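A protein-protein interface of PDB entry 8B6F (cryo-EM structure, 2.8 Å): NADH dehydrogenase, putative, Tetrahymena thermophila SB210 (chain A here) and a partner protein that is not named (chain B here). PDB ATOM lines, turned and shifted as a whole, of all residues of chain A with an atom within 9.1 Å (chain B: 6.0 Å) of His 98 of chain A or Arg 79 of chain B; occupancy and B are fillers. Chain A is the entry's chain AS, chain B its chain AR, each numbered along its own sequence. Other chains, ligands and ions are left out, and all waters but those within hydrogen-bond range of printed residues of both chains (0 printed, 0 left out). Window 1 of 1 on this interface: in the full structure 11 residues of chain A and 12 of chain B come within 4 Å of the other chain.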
ATOM      1  N   MET A  49     -26.833  -0.720   3.765  1.00  0.00           N
ATOM      2  CA  MET A  49     -25.666  -1.532   4.087  1.00  0.00           C
ATOM      3  C   MET A  49     -24.512  -0.666   4.566  1.00  0.00           C
ATOM      4  O   MET A  49     -23.648  -1.140   5.313  1.00  0.00           O
ATOM      5  CB  MET A  49     -25.243  -2.350   2.867  1.00  0.00           C
ATOM      6  CG  MET A  49     -26.132  -3.546   2.578  1.00  0.00           C
ATOM      7  SD  MET A  49     -26.237  -4.696   3.963  1.00  0.00           S
ATOM      8  CE  MET A  49     -24.505  -5.015   4.285  1.00  0.00           C
ATOM      9  N   TYR A  92     -13.916 -14.335  12.878  1.00  0.00           N
ATOM     10  CA  TYR A  92     -15.318 -14.629  13.146  1.00  0.00           C
ATOM     11  C   TYR A  92     -16.229 -13.684  12.371  1.00  0.00           C
ATOM     12  O   TYR A  92     -17.218 -14.117  11.770  1.00  0.00           O
ATOM     13  CB  TYR A  92     -15.585 -14.534  14.649  1.00  0.00           C
ATOM     14  CG  TYR A  92     -17.002 -14.869  15.045  1.00  0.00           C
ATOM     15  CD1 TYR A  92     -17.991 -13.898  15.061  1.00  0.00           C
ATOM     16  CD2 TYR A  92     -17.345 -16.161  15.416  1.00  0.00           C
ATOM     17  CE1 TYR A  92     -19.286 -14.206  15.425  1.00  0.00           C
ATOM     18  CE2 TYR A  92     -18.635 -16.480  15.782  1.00  0.00           C
ATOM     19  CZ  TYR A  92     -19.601 -15.499  15.786  1.00  0.00           C
ATOM     20  OH  TYR A  92     -20.888 -15.814  16.150  1.00  0.00           O
ATOM     21  N   ILE A  93     -15.911 -12.388  12.373  1.00  0.00           N
ATOM     22  CA  ILE A  93     -16.720 -11.417  11.641  1.00  0.00           C
ATOM     23  C   ILE A  93     -16.581 -11.630  10.139  1.00  0.00           C
ATOM     24  O   ILE A  93     -17.551 -11.482   9.388  1.00  0.00           O
ATOM     25  CB  ILE A  93     -16.338  -9.983  12.048  1.00  0.00           C
ATOM     26  CG1 ILE A  93     -16.728  -9.738  13.507  1.00  0.00           C
ATOM     27  CG2 ILE A  93     -17.013  -8.965  11.125  1.00  0.00           C
ATOM     28  CD1 ILE A  93     -16.381  -8.364  14.018  1.00  0.00           C
ATOM     29  N   ARG A  94     -15.378 -11.972   9.676  1.00  0.00           N
ATOM     30  CA  ARG A  94     -15.175 -12.187   8.246  1.00  0.00           C
ATOM     31  C   ARG A  94     -16.049 -13.322   7.733  1.00  0.00           C
ATOM     32  O   ARG A  94     -16.602 -13.240   6.631  1.00  0.00           O
ATOM     33  CB  ARG A  94     -13.704 -12.480   7.961  1.00  0.00           C
ATOM     34  CG  ARG A  94     -12.796 -11.266   8.047  1.00  0.00           C
ATOM     35  CD  ARG A  94     -11.348 -11.652   7.794  1.00  0.00           C
ATOM     36  NE  ARG A  94     -10.443 -10.521   7.965  1.00  0.00           N
ATOM     37  CZ  ARG A  94      -9.837 -10.200   9.100  1.00  0.00           C
ATOM     38  NH1 ARG A  94     -10.012 -10.906  10.205  1.00  0.00           N
ATOM     39  NH2 ARG A  94      -9.029  -9.144   9.127  1.00  0.00           N
ATOM     40  N   GLU A  95     -16.181 -14.394   8.511  1.00  0.00           N
ATOM     41  CA  GLU A  95     -17.057 -15.487   8.108  1.00  0.00           C
ATOM     42  C   GLU A  95     -18.491 -15.009   7.911  1.00  0.00           C
ATOM     43  O   GLU A  95     -19.231 -15.589   7.110  1.00  0.00           O
ATOM     44  CB  GLU A  95     -17.005 -16.604   9.145  1.00  0.00           C
ATOM     45  CG  GLU A  95     -15.714 -17.392   9.109  1.00  0.00           C
ATOM     46  CD  GLU A  95     -15.712 -18.536  10.093  1.00  0.00           C
ATOM     47  OE1 GLU A  95     -16.316 -18.388  11.176  1.00  0.00           O
ATOM     48  OE2 GLU A  95     -15.114 -19.586   9.782  1.00  0.00           O
ATOM     49  N   ARG A  96     -18.899 -13.964   8.628  1.00  0.00           N
ATOM     50  CA  ARG A  96     -20.243 -13.410   8.519  1.00  0.00           C
ATOM     51  C   ARG A  96     -20.309 -12.167   7.640  1.00  0.00           C
ATOM     52  O   ARG A  96     -21.384 -11.570   7.522  1.00  0.00           O
ATOM     53  CB  ARG A  96     -20.788 -13.069   9.912  1.00  0.00           C
ATOM     54  CG  ARG A  96     -21.318 -14.260  10.701  1.00  0.00           C
ATOM     55  CD  ARG A  96     -20.196 -15.141  11.226  1.00  0.00           C
ATOM     56  NE  ARG A  96     -20.701 -16.237  12.045  1.00  0.00           N
ATOM     57  CZ  ARG A  96     -19.942 -17.182  12.581  1.00  0.00           C
ATOM     58  NH1 ARG A  96     -18.630 -17.199  12.406  1.00  0.00           N
ATOM     59  NH2 ARG A  96     -20.512 -18.140  13.307  1.00  0.00           N
ATOM     60  N   ASN A  97     -19.203 -11.760   7.020  1.00  0.00           N
ATOM     61  CA  ASN A  97     -19.196 -10.517   6.257  1.00  0.00           C
ATOM     62  C   ASN A  97     -20.071 -10.579   5.012  1.00  0.00           C
ATOM     63  O   ASN A  97     -20.296  -9.539   4.385  1.00  0.00           O
ATOM     64  CB  ASN A  97     -17.766 -10.140   5.861  1.00  0.00           C
ATOM     65  CG  ASN A  97     -17.150 -11.119   4.884  1.00  0.00           C
ATOM     66  OD1 ASN A  97     -17.805 -12.051   4.419  1.00  0.00           O
ATOM     67  ND2 ASN A  97     -15.880 -10.908   4.562  1.00  0.00           N
ATOM     68  N   HIS A  98     -20.546 -11.763   4.622  1.00  0.00           N
ATOM     69  CA  HIS A  98     -21.372 -11.886   3.427  1.00  0.00           C
ATOM     70  C   HIS A  98     -22.793 -11.378   3.630  1.00  0.00           C
ATOM     71  O   HIS A  98     -23.546 -11.305   2.656  1.00  0.00           O
ATOM     72  CB  HIS A  98     -21.416 -13.343   2.968  1.00  0.00           C
ATOM     73  CG  HIS A  98     -22.069 -14.265   3.950  1.00  0.00           C
ATOM     74  ND1 HIS A  98     -21.375 -14.881   4.969  1.00  0.00           N
ATOM     75  CD2 HIS A  98     -23.351 -14.679   4.064  1.00  0.00           C
ATOM     76  CE1 HIS A  98     -22.205 -15.631   5.671  1.00  0.00           C
ATOM     77  NE2 HIS A  98     -23.411 -15.527   5.142  1.00  0.00           N
ATOM     78  N   TYR A  99     -23.176 -11.029   4.857  1.00  0.00           N
ATOM     79  CA  TYR A  99     -24.536 -10.577   5.112  1.00  0.00           C
ATOM     80  C   TYR A  99     -24.855  -9.340   4.284  1.00  0.00           C
ATOM     81  O   TYR A  99     -24.003  -8.473   4.074  1.00  0.00           O
ATOM     82  CB  TYR A  99     -24.726 -10.266   6.598  1.00  0.00           C
ATOM     83  CG  TYR A  99     -24.627 -11.461   7.517  1.00  0.00           C
ATOM     84  CD1 TYR A  99     -24.490 -12.748   7.017  1.00  0.00           C
ATOM     85  CD2 TYR A  99     -24.683 -11.298   8.894  1.00  0.00           C
ATOM     86  CE1 TYR A  99     -24.404 -13.836   7.860  1.00  0.00           C
ATOM     87  CE2 TYR A  99     -24.597 -12.378   9.746  1.00  0.00           C
ATOM     88  CZ  TYR A  99     -24.457 -13.645   9.223  1.00  0.00           C
ATOM     89  OH  TYR A  99     -24.373 -14.726  10.068  1.00  0.00           O
ATOM     90  N   ARG A 100     -26.100  -9.266   3.806  1.00  0.00           N
ATOM     91  CA  ARG A 100     -26.573  -8.120   3.039  1.00  0.00           C
ATOM     92  C   ARG A 100     -27.976  -7.705   3.468  1.00  0.00           C
ATOM     93  O   ARG A 100     -28.729  -7.137   2.671  1.00  0.00           O
ATOM     94  CB  ARG A 100     -26.558  -8.420   1.540  1.00  0.00           C
ATOM     95  CG  ARG A 100     -25.167  -8.533   0.944  1.00  0.00           C
ATOM     96  CD  ARG A 100     -24.469  -7.184   0.913  1.00  0.00           C
ATOM     97  NE  ARG A 100     -23.189  -7.249   0.220  1.00  0.00           N
ATOM     98  CZ  ARG A 100     -22.042  -7.599   0.786  1.00  0.00           C
ATOM     99  NH1 ARG A 100     -21.973  -7.931   2.064  1.00  0.00           N
ATOM    100  NH2 ARG A 100     -20.935  -7.617   0.050  1.00  0.00           N
ATOM    101  N   ASP A 101     -28.341  -7.984   4.713  1.00  0.00           N
ATOM    102  CA  ASP A 101     -29.657  -7.633   5.245  1.00  0.00           C
ATOM    103  C   ASP A 101     -29.488  -6.689   6.428  1.00  0.00           C
ATOM    104  O   ASP A 101     -29.024  -7.125   7.499  1.00  0.00           O
ATOM    105  CB  ASP A 101     -30.410  -8.894   5.666  1.00  0.00           C
ATOM    106  CG  ASP A 101     -31.883  -8.645   5.895  1.00  0.00           C
ATOM    107  OD1 ASP A 101     -32.313  -7.476   5.804  1.00  0.00           O
ATOM    108  OD2 ASP A 101     -32.616  -9.619   6.161  1.00  0.00           O
ATOM    109  N   LEU A 104     -31.046  -8.017   9.780  1.00  0.00           N
ATOM    110  CA  LEU A 104     -30.285  -9.117  10.359  1.00  0.00           C
ATOM    111  C   LEU A 104     -28.982  -8.620  10.972  1.00  0.00           C
ATOM    112  O   LEU A 104     -28.579  -9.072  12.049  1.00  0.00           O
ATOM    113  CB  LEU A 104     -30.006 -10.175   9.293  1.00  0.00           C
ATOM    114  CG  LEU A 104     -29.294 -11.440   9.770  1.00  0.00           C
ATOM    115  CD1 LEU A 104     -30.134 -12.190  10.789  1.00  0.00           C
ATOM    116  CD2 LEU A 104     -28.967 -12.331   8.587  1.00  0.00           C
ATOM    117  N   ILE A 105     -28.314  -7.683  10.300  1.00  0.00           N
ATOM    118  CA  ILE A 105     -27.068  -7.134  10.828  1.00  0.00           C
ATOM    119  C   ILE A 105     -27.320  -6.403  12.139  1.00  0.00           C
ATOM    120  O   ILE A 105     -26.547  -6.532  13.095  1.00  0.00           O
ATOM    121  CB  ILE A 105     -26.403  -6.219   9.785  1.00  0.00           C
ATOM    122  CG1 ILE A 105     -25.985  -7.040   8.563  1.00  0.00           C
ATOM    123  CG2 ILE A 105     -25.193  -5.525  10.397  1.00  0.00           C
ATOM    124  CD1 ILE A 105     -25.621  -6.209   7.360  1.00  0.00           C
ATOM    125  N   ARG A 108     -27.748  -8.955  14.810  1.00  0.00           N
ATOM    126  CA  ARG A 108     -26.453  -9.537  15.151  1.00  0.00           C
ATOM    127  C   ARG A 108     -25.625  -8.591  16.012  1.00  0.00           C
ATOM    128  O   ARG A 108     -24.955  -9.026  16.955  1.00  0.00           O
ATOM    129  CB  ARG A 108     -25.692  -9.897  13.876  1.00  0.00           C
ATOM    130  CG  ARG A 108     -26.305 -11.038  13.085  1.00  0.00           C
ATOM    131  CD  ARG A 108     -26.147 -12.364  13.811  1.00  0.00           C
ATOM    132  NE  ARG A 108     -26.584 -13.485  12.987  1.00  0.00           N
ATOM    133  CZ  ARG A 108     -27.841 -13.894  12.883  1.00  0.00           C
ATOM    134  NH1 ARG A 108     -28.821 -13.296  13.540  1.00  0.00           N
ATOM    135  NH2 ARG A 108     -28.122 -14.928  12.094  1.00  0.00           N
ATOM    136  N   LEU B  61     -23.478 -21.271  -0.885  1.00  0.00           N
ATOM    137  CA  LEU B  61     -22.867 -20.488   0.187  1.00  0.00           C
ATOM    138  C   LEU B  61     -22.604 -19.094  -0.360  1.00  0.00           C
ATOM    139  O   LEU B  61     -21.533 -18.797  -0.889  1.00  0.00           O
ATOM    140  CB  LEU B  61     -21.591 -21.152   0.690  1.00  0.00           C
ATOM    141  CG  LEU B  61     -21.707 -22.532   1.353  1.00  0.00           C
ATOM    142  CD1 LEU B  61     -22.799 -22.544   2.414  1.00  0.00           C
ATOM    143  CD2 LEU B  61     -21.942 -23.639   0.334  1.00  0.00           C
ATOM    144  N   ASP B  62     -23.600 -18.225  -0.222  1.00  0.00           N
ATOM    145  CA  ASP B  62     -23.569 -16.895  -0.809  1.00  0.00           C
ATOM    146  C   ASP B  62     -24.159 -15.928   0.209  1.00  0.00           C
ATOM    147  O   ASP B  62     -24.346 -16.271   1.380  1.00  0.00           O
ATOM    148  CB  ASP B  62     -24.336 -16.894  -2.138  1.00  0.00           C
ATOM    149  CG  ASP B  62     -23.915 -15.770  -3.057  1.00  0.00           C
ATOM    150  OD1 ASP B  62     -23.485 -14.717  -2.545  1.00  0.00           O
ATOM    151  OD2 ASP B  62     -24.017 -15.938  -4.291  1.00  0.00           O
ATOM    152  N   SER B  63     -24.455 -14.704  -0.230  1.00  0.00           N
ATOM    153  CA  SER B  63     -25.141 -13.766   0.646  1.00  0.00           C
ATOM    154  C   SER B  63     -26.578 -14.182   0.923  1.00  0.00           C
ATOM    155  O   SER B  63     -27.192 -13.644   1.850  1.00  0.00           O
ATOM    156  CB  SER B  63     -25.120 -12.361   0.042  1.00  0.00           C
ATOM    157  OG  SER B  63     -25.804 -12.330  -1.198  1.00  0.00           O
ATOM    158  N   SER B  64     -27.123 -15.121   0.148  1.00  0.00           N
ATOM    159  CA  SER B  64     -28.512 -15.523   0.318  1.00  0.00           C
ATOM    160  C   SER B  64     -28.710 -16.405   1.542  1.00  0.00           C
ATOM    161  O   SER B  64     -29.813 -16.444   2.097  1.00  0.00           O
ATOM    162  CB  SER B  64     -29.005 -16.250  -0.934  1.00  0.00           C
ATOM    163  OG  SER B  64     -28.274 -17.443  -1.152  1.00  0.00           O
ATOM    164  N   CYS B  65     -27.667 -17.118   1.978  1.00  0.00           N
ATOM    165  CA  CYS B  65     -27.767 -18.023   3.116  1.00  0.00           C
ATOM    166  C   CYS B  65     -27.413 -17.343   4.433  1.00  0.00           C
ATOM    167  O   CYS B  65     -26.965 -18.010   5.374  1.00  0.00           O
ATOM    168  CB  CYS B  65     -26.875 -19.246   2.894  1.00  0.00           C
ATOM    169  SG  CYS B  65     -25.118 -18.958   3.182  1.00  0.00           S
ATOM    170  N   GLN B  66     -27.605 -16.028   4.521  1.00  0.00           N
ATOM    171  CA  GLN B  66     -27.278 -15.290   5.734  1.00  0.00           C
ATOM    172  C   GLN B  66     -28.222 -15.603   6.888  1.00  0.00           C
ATOM    173  O   GLN B  66     -27.877 -15.332   8.043  1.00  0.00           O
ATOM    174  CB  GLN B  66     -27.298 -13.788   5.445  1.00  0.00           C
ATOM    175  CG  GLN B  66     -28.607 -13.288   4.856  1.00  0.00           C
ATOM    176  CD  GLN B  66     -28.549 -11.829   4.470  1.00  0.00           C
ATOM    177  OE1 GLN B  66     -27.849 -11.038   5.096  1.00  0.00           O
ATOM    178  NE2 GLN B  66     -29.283 -11.464   3.427  1.00  0.00           N
ATOM    179  N   THR B  68     -29.196 -18.487   8.060  1.00  0.00           N
ATOM    180  CA  THR B  68     -28.946 -19.728   8.778  1.00  0.00           C
ATOM    181  C   THR B  68     -28.485 -19.440  10.202  1.00  0.00           C
ATOM    182  O   THR B  68     -27.766 -18.471  10.455  1.00  0.00           O
ATOM    183  CB  THR B  68     -27.891 -20.561   8.050  1.00  0.00           C
ATOM    184  OG1 THR B  68     -27.748 -21.831   8.699  1.00  0.00           O
ATOM    185  CG2 THR B  68     -26.544 -19.846   8.041  1.00  0.00           C
ATOM    186  N   PHE B  70     -27.346 -22.327  12.059  1.00  0.00           N
ATOM    187  CA  PHE B  70     -26.598 -23.531  12.399  1.00  0.00           C
ATOM    188  C   PHE B  70     -25.128 -23.433  12.012  1.00  0.00           C
ATOM    189  O   PHE B  70     -24.507 -24.444  11.670  1.00  0.00           O
ATOM    190  CB  PHE B  70     -27.240 -24.750  11.741  1.00  0.00           C
ATOM    191  CG  PHE B  70     -28.663 -24.978  12.156  1.00  0.00           C
ATOM    192  CD1 PHE B  70     -28.956 -25.515  13.399  1.00  0.00           C
ATOM    193  CD2 PHE B  70     -29.705 -24.661  11.305  1.00  0.00           C
ATOM    194  CE1 PHE B  70     -30.264 -25.727  13.784  1.00  0.00           C
ATOM    195  CE2 PHE B  70     -31.014 -24.870  11.684  1.00  0.00           C
ATOM    196  CZ  PHE B  70     -31.294 -25.405  12.925  1.00  0.00           C
ATOM    197  N   TYR B  71     -24.561 -22.231  12.054  1.00  0.00           N
ATOM    198  CA  TYR B  71     -23.132 -22.014  11.853  1.00  0.00           C
ATOM    199  C   TYR B  71     -22.616 -21.340  13.119  1.00  0.00           C
ATOM    200  O   TYR B  71     -22.678 -20.117  13.258  1.00  0.00           O
ATOM    201  CB  TYR B  71     -22.859 -21.179  10.610  1.00  0.00           C
ATOM    202  CG  TYR B  71     -21.410 -21.195  10.185  1.00  0.00           C
ATOM    203  CD1 TYR B  71     -20.848 -22.330   9.613  1.00  0.00           C
ATOM    204  CD2 TYR B  71     -20.605 -20.077  10.351  1.00  0.00           C
ATOM    205  CE1 TYR B  71     -19.525 -22.351   9.223  1.00  0.00           C
ATOM    206  CE2 TYR B  71     -19.280 -20.089   9.965  1.00  0.00           C
ATOM    207  CZ  TYR B  71     -18.746 -21.228   9.401  1.00  0.00           C
ATOM    208  OH  TYR B  71     -17.428 -21.244   9.012  1.00  0.00           O
ATOM    209  N   ARG B  76     -19.823 -26.629  12.807  1.00  0.00           N
ATOM    210  CA  ARG B  76     -19.583 -25.980  11.524  1.00  0.00           C
ATOM    211  C   ARG B  76     -19.807 -26.940  10.359  1.00  0.00           C
ATOM    212  O   ARG B  76     -19.252 -26.725   9.275  1.00  0.00           O
ATOM    213  CB  ARG B  76     -18.162 -25.410  11.470  1.00  0.00           C
ATOM    214  CG  ARG B  76     -17.096 -26.385  11.940  1.00  0.00           C
ATOM    215  CD  ARG B  76     -15.738 -25.716  12.057  1.00  0.00           C
ATOM    216  NE  ARG B  76     -14.806 -26.534  12.824  1.00  0.00           N
ATOM    217  CZ  ARG B  76     -14.744 -26.557  14.148  1.00  0.00           C
ATOM    218  NH1 ARG B  76     -15.549 -25.816  14.893  1.00  0.00           N
ATOM    219  NH2 ARG B  76     -13.852 -27.345  14.742  1.00  0.00           N
ATOM    220  N   ASP B  77     -20.603 -27.993  10.560  1.00  0.00           N
ATOM    221  CA  ASP B  77     -20.892 -28.971   9.522  1.00  0.00           C
ATOM    222  C   ASP B  77     -22.333 -28.940   9.038  1.00  0.00           C
ATOM    223  O   ASP B  77     -22.612 -29.465   7.956  1.00  0.00           O
ATOM    224  CB  ASP B  77     -20.575 -30.387  10.026  1.00  0.00           C
ATOM    225  CG  ASP B  77     -21.281 -30.710  11.329  1.00  0.00           C
ATOM    226  OD1 ASP B  77     -21.963 -29.816  11.870  1.00  0.00           O
ATOM    227  OD2 ASP B  77     -21.152 -31.853  11.816  1.00  0.00           O
ATOM    228  N   ILE B  78     -23.249 -28.349   9.806  1.00  0.00           N
ATOM    229  CA  ILE B  78     -24.657 -28.341   9.416  1.00  0.00           C
ATOM    230  C   ILE B  78     -24.842 -27.568   8.116  1.00  0.00           C
ATOM    231  O   ILE B  78     -25.496 -28.041   7.180  1.00  0.00           O
ATOM    232  CB  ILE B  78     -25.522 -27.762  10.549  1.00  0.00           C
ATOM    233  CG1 ILE B  78     -25.441 -28.660  11.786  1.00  0.00           C
ATOM    234  CG2 ILE B  78     -26.968 -27.616  10.092  1.00  0.00           C
ATOM    235  CD1 ILE B  78     -26.010 -28.033  13.039  1.00  0.00           C
ATOM    236  N   ARG B  79     -24.272 -26.369   8.038  1.00  0.00           N
ATOM    237  CA  ARG B  79     -24.416 -25.563   6.835  1.00  0.00           C
ATOM    238  C   ARG B  79     -23.680 -26.215   5.673  1.00  0.00           C
ATOM    239  O   ARG B  79     -22.620 -26.822   5.847  1.00  0.00           O
ATOM    240  CB  ARG B  79     -23.883 -24.151   7.067  1.00  0.00           C
ATOM    241  CG  ARG B  79     -24.211 -23.192   5.933  1.00  0.00           C
ATOM    242  CD  ARG B  79     -23.637 -21.810   6.178  1.00  0.00           C
ATOM    243  NE  ARG B  79     -22.179 -21.819   6.191  1.00  0.00           N
ATOM    244  CZ  ARG B  79     -21.424 -20.735   6.293  1.00  0.00           C
ATOM    245  NH1 ARG B  79     -21.955 -19.528   6.388  1.00  0.00           N
ATOM    246  NH2 ARG B  79     -20.100 -20.865   6.300  1.00  0.00           N
ATOM    247  N   GLY B  80     -24.251 -26.085   4.478  1.00  0.00           N
ATOM    248  CA  GLY B  80     -23.688 -26.697   3.296  1.00  0.00           C
ATOM    249  C   GLY B  80     -24.042 -28.154   3.104  1.00  0.00           C
ATOM    250  O   GLY B  80     -23.619 -28.749   2.106  1.00  0.00           O
ATOM    251  N   ARG B  81     -24.798 -28.749   4.021  1.00  0.00           N
ATOM    252  CA  ARG B  81     -25.205 -30.136   3.871  1.00  0.00           C
ATOM    253  C   ARG B  81     -26.266 -30.250   2.781  1.00  0.00           C
ATOM    254  O   ARG B  81     -26.886 -29.264   2.373  1.00  0.00           O
ATOM    255  CB  ARG B  81     -25.735 -30.678   5.200  1.00  0.00           C
ATOM    256  CG  ARG B  81     -25.657 -32.192   5.325  1.00  0.00           C
ATOM    257  CD  ARG B  81     -26.163 -32.677   6.677  1.00  0.00           C
ATOM    258  NE  ARG B  81     -25.386 -32.142   7.789  1.00  0.00           N
ATOM    259  CZ  ARG B  81     -25.522 -32.527   9.050  1.00  0.00           C
ATOM    260  NH1 ARG B  81     -26.388 -33.465   9.398  1.00  0.00           N
ATOM    261  NH2 ARG B  81     -24.770 -31.959   9.988  1.00  0.00           N
ATOM    262  N   MET B 149     -31.209 -21.121   4.143  1.00  0.00           N
ATOM    263  CA  MET B 149     -30.324 -21.732   5.125  1.00  0.00           C
ATOM    264  C   MET B 149     -29.022 -22.250   4.526  1.00  0.00           C
ATOM    265  O   MET B 149     -28.179 -22.761   5.269  1.00  0.00           O
ATOM    266  CB  MET B 149     -31.049 -22.877   5.838  1.00  0.00           C
ATOM    267  CG  MET B 149     -32.355 -22.456   6.491  1.00  0.00           C
ATOM    268  SD  MET B 149     -32.167 -21.066   7.622  1.00  0.00           S
ATOM    269  CE  MET B 149     -33.879 -20.680   7.977  1.00  0.00           C
ATOM    270  N   GLY B 150     -28.834 -22.127   3.215  1.00  0.00           N
ATOM    271  CA  GLY B 150     -27.579 -22.512   2.603  1.00  0.00           C
ATOM    272  C   GLY B 150     -27.370 -24.001   2.457  1.00  0.00           C
ATOM    273  O   GLY B 150     -26.224 -24.443   2.336  1.00  0.00           O
ATOM    274  N   PHE B 151     -28.437 -24.792   2.475  1.00  0.00           N
ATOM    275  CA  PHE B 151     -28.345 -26.226   2.251  1.00  0.00           C
ATOM    276  C   PHE B 151     -28.521 -26.542   0.773  1.00  0.00           C
ATOM    277  O   PHE B 151     -29.359 -25.944   0.094  1.00  0.00           O
ATOM    278  CB  PHE B 151     -29.414 -26.974   3.052  1.00  0.00           C
ATOM    279  CG  PHE B 151     -29.343 -26.749   4.532  1.00  0.00           C
ATOM    280  CD1 PHE B 151     -28.128 -26.756   5.193  1.00  0.00           C
ATOM    281  CD2 PHE B 151     -30.497 -26.533   5.262  1.00  0.00           C
ATOM    282  CE1 PHE B 151     -28.067 -26.550   6.556  1.00  0.00           C
ATOM    283  CE2 PHE B 151     -30.443 -26.326   6.624  1.00  0.00           C
ATOM    284  CZ  PHE B 151     -29.227 -26.336   7.272  1.00  0.00           C
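Hydrophobic or aromatic side chains of chain A that line the printed part of chain B: His 98, Tyr 99 and Leu 104.
Of the 18 printed residues of chain B, 6 touch a printed residue of chain A.
Hydrophobic or aromatic side chains of chain B that line the printed part of chain A: Tyr 71.
Along chain B the printed residues that touch a printed residue of chain A span positions 62 to 79.
Among the printed residues, no Asp or Glu carboxylate lies within 4 Å of a Lys or Arg side-chain nitrogen of the other chain.
Among the printed residues, merely in contact across the chains: His 98 of chain A with Asp 62 of chain B (3.3 Å), His 98 of chain A with Ser 63 of chain B (3.2 Å), His 98 of chain A with Gln 66 of chain B (3.9 Å), His 98 of chain A with Arg 79 of chain B (3.97 Å), Tyr 99 of chain A with Gln 66 of chain B (3.3 Å), Arg 100 of chain A with Ser 63 of chain B (3.9 Å), Leu 104 of chain A with Gln 66 of chain B (3.2 Å) and Arg 108 of chain A with Thr 68 of chain B (3.9 Å).
OE1 of Gln 66 of chain B sits at hydrogen-bond distance from N of Asp 101 of chain A, 3.1 Å away.
The backbone carbonyl oxygen (O) of Tyr 71 of chain B is in hydrogen-bond range of the guanidinium group (NH2) of Arg 96 of chain A (2.9 Å).
The side-chain carboxylate (OE2) of Glu 95 of chain A lies within hydrogen-bond range of the side-chain hydroxyl (OH) of Tyr 71 of chain B (2.9 Å).
The side-chain amide oxygen of Gln 66 of chain B sits at hydrogen-bond distance from the backbone NH of Arg 100 of chain A (2.8 Å).
His 98 of chain A touches just these residues of chain B: Asp 62, Ser 63, Gln 66 and Arg 79.
Printed residues of chain A within 4 Å of Arg 79 of chain B: His 98.
Ser 63 of chain B touches two residues of chain A.
Printed residues of chain A within 4 Å of Tyr 71 of chain B: Glu 95 (2.9 Å) and Arg 96 (2.9 Å).
Of the printed residues of chain A, Thr 68 of chain B touches Arg 108.
Of the printed residues of chain B, Asp 101 of chain A touches Gln 66 (3.1 Å).
Of the printed residues of chain B, Arg 108 of chain A touches Thr 68 (3.9 Å).
Printed residues of chain B within 4 Å of Arg 100 of chain A: Ser 63 and Gln 66.
Asp 77 of chain B touches none of the printed residues of chain A.
Ile 105 of chain A touches none of the printed residues of chain B.
The backbone carbonyl oxygen (O) of Ser 63 of chain B sits close to the side-chain amide nitrogen (NE2) of Gln 66 of chain B.
N of Phe 70 of chain B lies within hydrogen-bond range of OG1 of Thr 68 of chain B.
OE1 of Glu 95 of chain A is in salt-bridge range of NH1 of Arg 96 of chain A (2.9 Å).
O of Glu 95 of chain A sits at hydrogen-bond distance from ND1 of His 98 of chain A, 3.1 Å away.
NH1 of Arg 100 of chain A sits at hydrogen-bond distance from O of Asn 97 of chain A, at 3.3 Å.
O of Asp 62 of chain B sits at hydrogen-bond distance from SG of Cys 65 of chain B (3.3 Å).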
